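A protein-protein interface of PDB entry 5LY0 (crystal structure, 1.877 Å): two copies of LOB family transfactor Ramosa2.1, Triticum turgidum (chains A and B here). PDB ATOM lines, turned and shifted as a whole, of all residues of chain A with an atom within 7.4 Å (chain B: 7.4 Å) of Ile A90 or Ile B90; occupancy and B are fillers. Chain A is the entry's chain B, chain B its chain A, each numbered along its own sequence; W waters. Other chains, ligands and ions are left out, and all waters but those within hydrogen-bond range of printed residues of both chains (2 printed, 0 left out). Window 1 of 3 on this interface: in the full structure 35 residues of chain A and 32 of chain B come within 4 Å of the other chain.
The side-chain carboxylate (OE2) of Glu B74 sits close to the side-chain carboxylate (OE1) of Glu A74. The side-chain sulfur (SG) of Cys B86 lies close to the side-chain carboxylate (OE1) of Glu A74 (3.8 Å). SG of Cys B86 sits at hydrogen-bond distance from SG of Cys A86, at 3.3 Å.
The side-chain hydroxyl (OG) of Ser B91 is in hydrogen-bond range of the backbone carbonyl oxygen (O) of Val B87 (3.1 Å). OG of Ser A91 sits at hydrogen-bond distance from O of Val A87 (3.3 Å).
Val B87 touches Tyr A73 (CG2 to CD1, 3.7 Å). Ile B90 touches Tyr A73. Glu A74 touches Val B87. CB of Cys A86 touches CD1 of Ile B90, at 3.9 Å. Val A87 touches Tyr B73. CD1 of Ile A90 touches CE1 of Tyr B73, at 3.5 Å. Ile A90 touches Cys B86. Ile B90 touches Ile A90 (CG1 to CG1, 3.7 Å). CD1 of Leu B93 touches CG2 of Ile A90 (3.9 Å). Leu A93 touches Leu B93 (CB to CB, 3.8 Å).
Of the printed residues of chain B, Ile A90 touches Tyr B73 (3.5 Å), Cys B86 (3.8 Å), Ile B90 (3.7 Å) and Leu B93 (3.9 Å). Ile B90 touches just these residues of chain A: Tyr A73 (3.5 Å), Cys A86 (3.9 Å) and Ile A90 (3.7 Å). No residue of chain A comes within 4 Å of Ala B89. Printed residues of chain B within 4 Å of Tyr A73: Val B87 and Ile B90. Of the printed residues of chain A, Leu B93 touches Ile A90 and Leu A93. Ala A77 touches none of the printed residues of chain B. Gln B94 touches none of the printed residues of chain A. The nearest printed residue of chain A that does not touch Cys B86 is Val A87 (5.4 Å).
Printed residues of chain A that touch a printed residue of chain B: Tyr A73, Glu A74, Cys A86, Val A87, Ile A90 and Leu A93. Printed residues of chain B that touch a printed residue of chain A: Tyr B73, Glu B74, Cys B86, Val B87, Ile B90 and Leu B93. Among the printed residues, 13 pairs touch across the chains.
Tyr A73 touches Val B87, and with the chains exchanged Val A87 touches Tyr B73. Glu A74 touches its own counterpart, Glu B74. Glu A74 touches Cys B86, but with the chains exchanged Cys A86 does not touch Glu B74 (4.2 Å). Cys A86 touches Ile B90, and with the chains exchanged Ile A90 touches Cys B86. Positions printed for both chains: 73, 74, 77, 85, 86, 87, 88, 89, 90, 91, 92, 93, 94, 95 and 96. Of the 13 pairs that touch across the chains among the printed residues, 10 have their exchanged pair printed and touching as well.
Water W1 lies within hydrogen-bond range of the backbone carbonyl oxygen (O) of Glu B74 (2.8 Å), the side-chain carboxylate (OE1) of Glu A74 (2.8 Å) and the backbone NH (N) of Cys B86 (2.9 Å). Water W2 lies within hydrogen-bond range of the backbone NH (N) of Cys A86 (2.8 Å), the backbone carbonyl oxygen (O) of Glu A74 (2.9 Å) and the side-chain carboxylate (OE2) of Glu B74 (3.0 Å).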
ATOM      1  N   TYR A  73      15.406  16.420 -20.642  1.00  0.00           N
ATOM      2  CA  TYR A  73      16.406  16.268 -19.592  1.00  0.00           C
ATOM      3  C   TYR A  73      17.291  15.054 -19.852  1.00  0.00           C
ATOM      4  O   TYR A  73      18.524  15.143 -19.786  1.00  0.00           O
ATOM      5  CB  TYR A  73      15.710  16.158 -18.234  1.00  0.00           C
ATOM      6  CG  TYR A  73      16.653  15.943 -17.075  1.00  0.00           C
ATOM      7  CD1 TYR A  73      17.123  14.674 -16.767  1.00  0.00           C
ATOM      8  CD2 TYR A  73      17.068  17.006 -16.286  1.00  0.00           C
ATOM      9  CE1 TYR A  73      17.982  14.468 -15.713  1.00  0.00           C
ATOM     10  CE2 TYR A  73      17.928  16.810 -15.224  1.00  0.00           C
ATOM     11  CZ  TYR A  73      18.380  15.539 -14.945  1.00  0.00           C
ATOM     12  OH  TYR A  73      19.238  15.331 -13.892  1.00  0.00           O
ATOM     13  N   GLU A  74      16.677  13.905 -20.147  1.00  0.00           N
ATOM     14  CA  GLU A  74      17.449  12.701 -20.435  1.00  0.00           C
ATOM     15  C   GLU A  74      18.348  12.897 -21.647  1.00  0.00           C
ATOM     16  O   GLU A  74      19.519  12.497 -21.632  1.00  0.00           O
ATOM     17  CB  GLU A  74      16.512  11.514 -20.671  1.00  0.00           C
ATOM     18  CG  GLU A  74      15.713  11.077 -19.459  1.00  0.00           C
ATOM     19  CD  GLU A  74      14.832   9.882 -19.759  1.00  0.00           C
ATOM     20  OE1 GLU A  74      15.325   8.906 -20.362  1.00  0.00           O
ATOM     21  OE2 GLU A  74      13.637   9.921 -19.404  1.00  0.00           O
ATOM     22  N   ALA A  77      21.383  15.092 -20.920  1.00  0.00           N
ATOM     23  CA  ALA A  77      22.353  14.336 -20.138  1.00  0.00           C
ATOM     24  C   ALA A  77      23.097  13.333 -21.011  1.00  0.00           C
ATOM     25  O   ALA A  77      24.294  13.093 -20.811  1.00  0.00           O
ATOM     26  CB  ALA A  77      21.651  13.630 -18.979  1.00  0.00           C
ATOM     27  N   GLY A  85      24.747   8.971 -19.523  1.00  0.00           N
ATOM     28  CA  GLY A  85      23.575   9.815 -19.487  1.00  0.00           C
ATOM     29  C   GLY A  85      23.232  10.172 -18.057  1.00  0.00           C
ATOM     30  O   GLY A  85      24.105  10.315 -17.194  1.00  0.00           O
ATOM     31  N   CYS A  86      21.938  10.297 -17.785  1.00  0.00           N
ATOM     32  CA  CYS A  86      21.510  10.647 -16.437  1.00  0.00           C
ATOM     33  C   CYS A  86      21.557   9.463 -15.478  1.00  0.00           C
ATOM     34  O   CYS A  86      21.288   9.642 -14.286  1.00  0.00           O
ATOM     35  CB  CYS A  86      20.105  11.243 -16.472  1.00  0.00           C
ATOM     36  SG  CYS A  86      18.874  10.185 -17.185  1.00  0.00           S
ATOM     37  N   VAL A  87      21.891   8.260 -15.958  1.00  0.00           N
ATOM     38  CA  VAL A  87      22.166   7.156 -15.042  1.00  0.00           C
ATOM     39  C   VAL A  87      23.363   7.497 -14.167  1.00  0.00           C
ATOM     40  O   VAL A  87      23.455   7.046 -13.018  1.00  0.00           O
ATOM     41  CB  VAL A  87      22.395   5.840 -15.818  1.00  0.00           C
ATOM     42  CG1 VAL A  87      22.670   4.690 -14.853  1.00  0.00           C
ATOM     43  CG2 VAL A  87      21.194   5.517 -16.699  1.00  0.00           C
ATOM     44  N   GLY A  88      24.298   8.291 -14.690  1.00  0.00           N
ATOM     45  CA  GLY A  88      25.412   8.742 -13.872  1.00  0.00           C
ATOM     46  C   GLY A  88      24.952   9.503 -12.644  1.00  0.00           C
ATOM     47  O   GLY A  88      25.440   9.277 -11.535  1.00  0.00           O
ATOM     48  N   ALA A  89      24.001  10.421 -12.828  1.00  0.00           N
ATOM     49  CA  ALA A  89      23.449  11.153 -11.693  1.00  0.00           C
ATOM     50  C   ALA A  89      22.807  10.205 -10.690  1.00  0.00           C
ATOM     51  O   ALA A  89      22.983  10.359  -9.475  1.00  0.00           O
ATOM     52  CB  ALA A  89      22.432  12.184 -12.181  1.00  0.00           C
ATOM     53  N   ILE A  90      22.058   9.214 -11.179  1.00  0.00           N
ATOM     54  CA  ILE A  90      21.406   8.261 -10.285  1.00  0.00           C
ATOM     55  C   ILE A  90      22.446   7.507  -9.466  1.00  0.00           C
ATOM     56  O   ILE A  90      22.288   7.324  -8.253  1.00  0.00           O
ATOM     57  CB  ILE A  90      20.509   7.304 -11.094  1.00  0.00           C
ATOM     58  CG1 ILE A  90      19.378   8.091 -11.761  1.00  0.00           C
ATOM     59  CG2 ILE A  90      19.932   6.212 -10.196  1.00  0.00           C
ATOM     60  CD1 ILE A  90      18.583   7.303 -12.775  1.00  0.00           C
ATOM     61  N   SER A  91      23.528   7.062 -10.111  1.00  0.00           N
ATOM     62  CA  SER A  91      24.593   6.374  -9.386  1.00  0.00           C
ATOM     63  C   SER A  91      25.199   7.273  -8.317  1.00  0.00           C
ATOM     64  O   SER A  91      25.419   6.836  -7.179  1.00  0.00           O
ATOM     65  CB  SER A  91      25.673   5.906 -10.360  1.00  0.00           C
ATOM     66  OG  SER A  91      25.193   4.878 -11.203  1.00  0.00           O
ATOM     67  N   VAL A  92      25.477   8.532  -8.661  1.00  0.00           N
ATOM     68  CA  VAL A  92      26.062   9.463  -7.700  1.00  0.00           C
ATOM     69  C   VAL A  92      25.125   9.655  -6.513  1.00  0.00           C
ATOM     70  O   VAL A  92      25.549   9.638  -5.351  1.00  0.00           O
ATOM     71  CB  VAL A  92      26.387  10.803  -8.389  1.00  0.00           C
ATOM     72  CG1 VAL A  92      26.715  11.889  -7.360  1.00  0.00           C
ATOM     73  CG2 VAL A  92      27.544  10.629  -9.361  1.00  0.00           C
ATOM     74  N   LEU A  93      23.835   9.849  -6.789  1.00  0.00           N
ATOM     75  CA  LEU A  93      22.880  10.101  -5.715  1.00  0.00           C
ATOM     76  C   LEU A  93      22.699   8.870  -4.836  1.00  0.00           C
ATOM     77  O   LEU A  93      22.586   8.987  -3.611  1.00  0.00           O
ATOM     78  CB  LEU A  93      21.544  10.549  -6.308  1.00  0.00           C
ATOM     79  CG  LEU A  93      21.586  11.920  -6.991  1.00  0.00           C
ATOM     80  CD1 LEU A  93      20.360  12.139  -7.867  1.00  0.00           C
ATOM     81  CD2 LEU A  93      21.703  13.027  -5.954  1.00  0.00           C
ATOM     82  N   GLN A  94      22.678   7.680  -5.439  1.00  0.00           N
ATOM     83  CA  GLN A  94      22.534   6.459  -4.651  1.00  0.00           C
ATOM     84  C   GLN A  94      23.713   6.271  -3.703  1.00  0.00           C
ATOM     85  O   GLN A  94      23.533   5.855  -2.552  1.00  0.00           O
ATOM     86  CB  GLN A  94      22.384   5.253  -5.579  1.00  0.00           C
ATOM     87  CG  GLN A  94      20.943   4.973  -5.982  1.00  0.00           C
ATOM     88  CD  GLN A  94      20.821   3.846  -6.990  1.00  0.00           C
ATOM     89  OE1 GLN A  94      21.790   3.485  -7.660  1.00  0.00           O
ATOM     90  NE2 GLN A  94      19.624   3.280  -7.100  1.00  0.00           N
ATOM     91  N   ARG A  95      24.929   6.570  -4.166  1.00  0.00           N
ATOM     92  CA  ARG A  95      26.091   6.490  -3.287  1.00  0.00           C
ATOM     93  C   ARG A  95      25.947   7.432  -2.100  1.00  0.00           C
ATOM     94  O   ARG A  95      26.287   7.075  -0.966  1.00  0.00           O
ATOM     95  CB  ARG A  95      27.367   6.816  -4.064  1.00  0.00           C
ATOM     96  CG  ARG A  95      27.881   5.684  -4.934  1.00  0.00           C
ATOM     97  CD  ARG A  95      28.915   6.181  -5.933  1.00  0.00           C
ATOM     98  NE  ARG A  95      28.993   5.323  -7.111  1.00  0.00           N
ATOM     99  CZ  ARG A  95      29.645   5.637  -8.225  1.00  0.00           C
ATOM    100  NH1 ARG A  95      30.283   6.797  -8.327  1.00  0.00           N
ATOM    101  NH2 ARG A  95      29.657   4.792  -9.244  1.00  0.00           N
ATOM    102  N   GLN A  96      25.440   8.642  -2.342  1.00  0.00           N
ATOM    103  CA  GLN A  96      25.334   9.629  -1.274  1.00  0.00           C
ATOM    104  C   GLN A  96      24.253   9.246  -0.272  1.00  0.00           C
ATOM    105  O   GLN A  96      24.406   9.479   0.933  1.00  0.00           O
ATOM    106  CB  GLN A  96      25.058  11.008  -1.865  1.00  0.00           C
ATOM    107  CG  GLN A  96      25.059  12.121  -0.840  1.00  0.00           C
ATOM    108  CD  GLN A  96      25.087  13.494  -1.473  1.00  0.00           C
ATOM    109  OE1 GLN A  96      24.998  13.630  -2.695  1.00  0.00           O
ATOM    110  NE2 GLN A  96      25.216  14.524  -0.645  1.00  0.00           N
ATOM    111  N   TYR B  73      18.973   0.396 -18.456  1.00  0.00           N
ATOM    112  CA  TYR B  73      18.313   0.924 -17.270  1.00  0.00           C
ATOM    113  C   TYR B  73      17.382   2.069 -17.637  1.00  0.00           C
ATOM    114  O   TYR B  73      16.249   2.145 -17.146  1.00  0.00           O
ATOM    115  CB  TYR B  73      19.352   1.391 -16.249  1.00  0.00           C
ATOM    116  CG  TYR B  73      18.732   2.075 -15.053  1.00  0.00           C
ATOM    117  CD1 TYR B  73      18.476   3.442 -15.064  1.00  0.00           C
ATOM    118  CD2 TYR B  73      18.394   1.355 -13.919  1.00  0.00           C
ATOM    119  CE1 TYR B  73      17.901   4.068 -13.977  1.00  0.00           C
ATOM    120  CE2 TYR B  73      17.820   1.974 -12.825  1.00  0.00           C
ATOM    121  CZ  TYR B  73      17.576   3.332 -12.860  1.00  0.00           C
ATOM    122  OH  TYR B  73      17.005   3.957 -11.776  1.00  0.00           O
ATOM    123  N   GLU B  74      17.842   2.967 -18.509  1.00  0.00           N
ATOM    124  CA  GLU B  74      17.040   4.124 -18.887  1.00  0.00           C
ATOM    125  C   GLU B  74      15.793   3.701 -19.654  1.00  0.00           C
ATOM    126  O   GLU B  74      14.708   4.257 -19.445  1.00  0.00           O
ATOM    127  CB  GLU B  74      17.896   5.083 -19.714  1.00  0.00           C
ATOM    128  CG  GLU B  74      17.302   6.459 -19.921  1.00  0.00           C
ATOM    129  CD  GLU B  74      18.321   7.444 -20.467  1.00  0.00           C
ATOM    130  OE1 GLU B  74      19.529   7.131 -20.449  1.00  0.00           O
ATOM    131  OE2 GLU B  74      17.909   8.535 -20.915  1.00  0.00           O
ATOM    132  N   ALA B  77      13.300   1.991 -17.293  1.00  0.00           N
ATOM    133  CA  ALA B  77      12.639   3.003 -16.478  1.00  0.00           C
ATOM    134  C   ALA B  77      11.521   3.696 -17.246  1.00  0.00           C
ATOM    135  O   ALA B  77      10.498   4.068 -16.657  1.00  0.00           O
ATOM    136  CB  ALA B  77      13.660   4.027 -15.983  1.00  0.00           C
ATOM    137  N   GLY B  85      10.146   8.537 -16.796  1.00  0.00           N
ATOM    138  CA  GLY B  85      11.305   7.679 -16.971  1.00  0.00           C
ATOM    139  C   GLY B  85      12.200   7.731 -15.751  1.00  0.00           C
ATOM    140  O   GLY B  85      11.738   7.821 -14.608  1.00  0.00           O
ATOM    141  N   CYS B  86      13.509   7.689 -15.988  1.00  0.00           N
ATOM    142  CA  CYS B  86      14.458   7.696 -14.887  1.00  0.00           C
ATOM    143  C   CYS B  86      14.612   9.072 -14.248  1.00  0.00           C
ATOM    144  O   CYS B  86      15.297   9.188 -13.226  1.00  0.00           O
ATOM    145  CB  CYS B  86      15.812   7.187 -15.379  1.00  0.00           C
ATOM    146  SG  CYS B  86      16.420   8.075 -16.821  1.00  0.00           S
ATOM    147  N   VAL B  87      13.988  10.110 -14.815  1.00  0.00           N
ATOM    148  CA  VAL B  87      13.988  11.412 -14.157  1.00  0.00           C
ATOM    149  C   VAL B  87      13.148  11.353 -12.890  1.00  0.00           C
ATOM    150  O   VAL B  87      13.400  12.095 -11.932  1.00  0.00           O
ATOM    151  CB  VAL B  87      13.488  12.514 -15.112  1.00  0.00           C
ATOM    152  CG1 VAL B  87      13.726  13.890 -14.503  1.00  0.00           C
ATOM    153  CG2 VAL B  87      14.173  12.413 -16.473  1.00  0.00           C
ATOM    154  N   GLY B  88      12.141  10.477 -12.858  1.00  0.00           N
ATOM    155  CA  GLY B  88      11.407  10.258 -11.624  1.00  0.00           C
ATOM    156  C   GLY B  88      12.297   9.731 -10.515  1.00  0.00           C
ATOM    157  O   GLY B  88      12.157  10.121  -9.352  1.00  0.00           O
ATOM    158  N   ALA B  89      13.232   8.842 -10.859  1.00  0.00           N
ATOM    159  CA  ALA B  89      14.190   8.353  -9.875  1.00  0.00           C
ATOM    160  C   ALA B  89      15.062   9.487  -9.354  1.00  0.00           C
ATOM    161  O   ALA B  89      15.329   9.573  -8.149  1.00  0.00           O
ATOM    162  CB  ALA B  89      15.056   7.252 -10.487  1.00  0.00           C
ATOM    163  N   ILE B  90      15.517  10.367 -10.250  1.00  0.00           N
ATOM    164  CA  ILE B  90      16.328  11.508  -9.837  1.00  0.00           C
ATOM    165  C   ILE B  90      15.541  12.401  -8.886  1.00  0.00           C
ATOM    166  O   ILE B  90      16.063  12.848  -7.857  1.00  0.00           O
ATOM    167  CB  ILE B  90      16.817  12.285 -11.075  1.00  0.00           C
ATOM    168  CG1 ILE B  90      17.778  11.417 -11.890  1.00  0.00           C
ATOM    169  CG2 ILE B  90      17.498  13.593 -10.668  1.00  0.00           C
ATOM    170  CD1 ILE B  90      18.105  11.974 -13.254  1.00  0.00           C
ATOM    171  N   SER B  91      14.277  12.680  -9.214  1.00  0.00           N
ATOM    172  CA  SER B  91      13.451  13.503  -8.337  1.00  0.00           C
ATOM    173  C   SER B  91      13.332  12.882  -6.951  1.00  0.00           C
ATOM    174  O   SER B  91      13.448  13.580  -5.936  1.00  0.00           O
ATOM    175  CB  SER B  91      12.064  13.699  -8.951  1.00  0.00           C
ATOM    176  OG  SER B  91      12.146  14.344 -10.210  1.00  0.00           O
ATOM    177  N   VAL B  92      13.099  11.567  -6.887  1.00  0.00           N
ATOM    178  CA  VAL B  92      12.985  10.893  -5.598  1.00  0.00           C
ATOM    179  C   VAL B  92      14.306  10.967  -4.843  1.00  0.00           C
ATOM    180  O   VAL B  92      14.337  11.232  -3.636  1.00  0.00           O
ATOM    181  CB  VAL B  92      12.529   9.434  -5.802  1.00  0.00           C
ATOM    182  CG1 VAL B  92      12.607   8.649  -4.494  1.00  0.00           C
ATOM    183  CG2 VAL B  92      11.113   9.397  -6.358  1.00  0.00           C
ATOM    184  N   LEU B  93      15.418  10.732  -5.541  1.00  0.00           N
ATOM    185  CA  LEU B  93      16.720  10.728  -4.882  1.00  0.00           C
ATOM    186  C   LEU B  93      17.115  12.125  -4.423  1.00  0.00           C
ATOM    187  O   LEU B  93      17.744  12.282  -3.368  1.00  0.00           O
ATOM    188  CB  LEU B  93      17.772  10.146  -5.823  1.00  0.00           C
ATOM    189  CG  LEU B  93      17.683   8.630  -5.991  1.00  0.00           C
ATOM    190  CD1 LEU B  93      18.396   8.183  -7.253  1.00  0.00           C
ATOM    191  CD2 LEU B  93      18.266   7.933  -4.768  1.00  0.00           C
ATOM    192  N   GLN B  94      16.764  13.154  -5.196  1.00  0.00           N
ATOM    193  CA  GLN B  94      17.017  14.524  -4.765  1.00  0.00           C
ATOM    194  C   GLN B  94      16.324  14.805  -3.439  1.00  0.00           C
ATOM    195  O   GLN B  94      16.922  15.368  -2.515  1.00  0.00           O
ATOM    196  CB  GLN B  94      16.549  15.506  -5.841  1.00  0.00           C
ATOM    197  CG  GLN B  94      16.641  16.981  -5.449  1.00  0.00           C
ATOM    198  CD  GLN B  94      15.924  17.891  -6.427  1.00  0.00           C
ATOM    199  OE1 GLN B  94      16.507  18.832  -6.965  1.00  0.00           O
ATOM    200  NE2 GLN B  94      14.642  17.623  -6.651  1.00  0.00           N
ATOM    201  N   ARG B  95      15.055  14.409  -3.327  1.00  0.00           N
ATOM    202  CA  ARG B  95      14.316  14.631  -2.090  1.00  0.00           C
ATOM    203  C   ARG B  95      14.933  13.854  -0.935  1.00  0.00           C
ATOM    204  O   ARG B  95      15.046  14.372   0.183  1.00  0.00           O
ATOM    205  CB  ARG B  95      12.852  14.229  -2.280  1.00  0.00           C
ATOM    206  CG  ARG B  95      11.883  15.035  -1.433  1.00  0.00           C
ATOM    207  CD  ARG B  95      10.490  14.417  -1.363  1.00  0.00           C
ATOM    208  NE  ARG B  95      10.175  13.548  -2.496  1.00  0.00           N
ATOM    209  CZ  ARG B  95      10.061  13.958  -3.755  1.00  0.00           C
ATOM    210  NH1 ARG B  95      10.262  15.230  -4.072  1.00  0.00           N
ATOM    211  NH2 ARG B  95       9.762  13.083  -4.708  1.00  0.00           N
ATOM    212  N   GLN B  96      15.345  12.611  -1.183  1.00  0.00           N
ATOM    213  CA  GLN B  96      15.820  11.761  -0.095  1.00  0.00           C
ATOM    214  C   GLN B  96      17.175  12.226   0.425  1.00  0.00           C
ATOM    215  O   GLN B  96      17.415  12.214   1.639  1.00  0.00           O
ATOM    216  CB  GLN B  96      15.892  10.306  -0.557  1.00  0.00           C
ATOM    217  CG  GLN B  96      16.202   9.315   0.556  1.00  0.00           C
ATOM    218  CD  GLN B  96      15.010   9.049   1.457  1.00  0.00           C
ATOM    219  OE1 GLN B  96      14.007   9.761   1.409  1.00  0.00           O
ATOM    220  NE2 GLN B  96      15.116   8.015   2.282  1.00  0.00           N
HETATM  221  O   HOH W   1      14.252   6.884 -18.687  1.00  0.00           O
HETATM  222  O   HOH W   2      20.296  10.143 -20.083  1.00  0.00           O
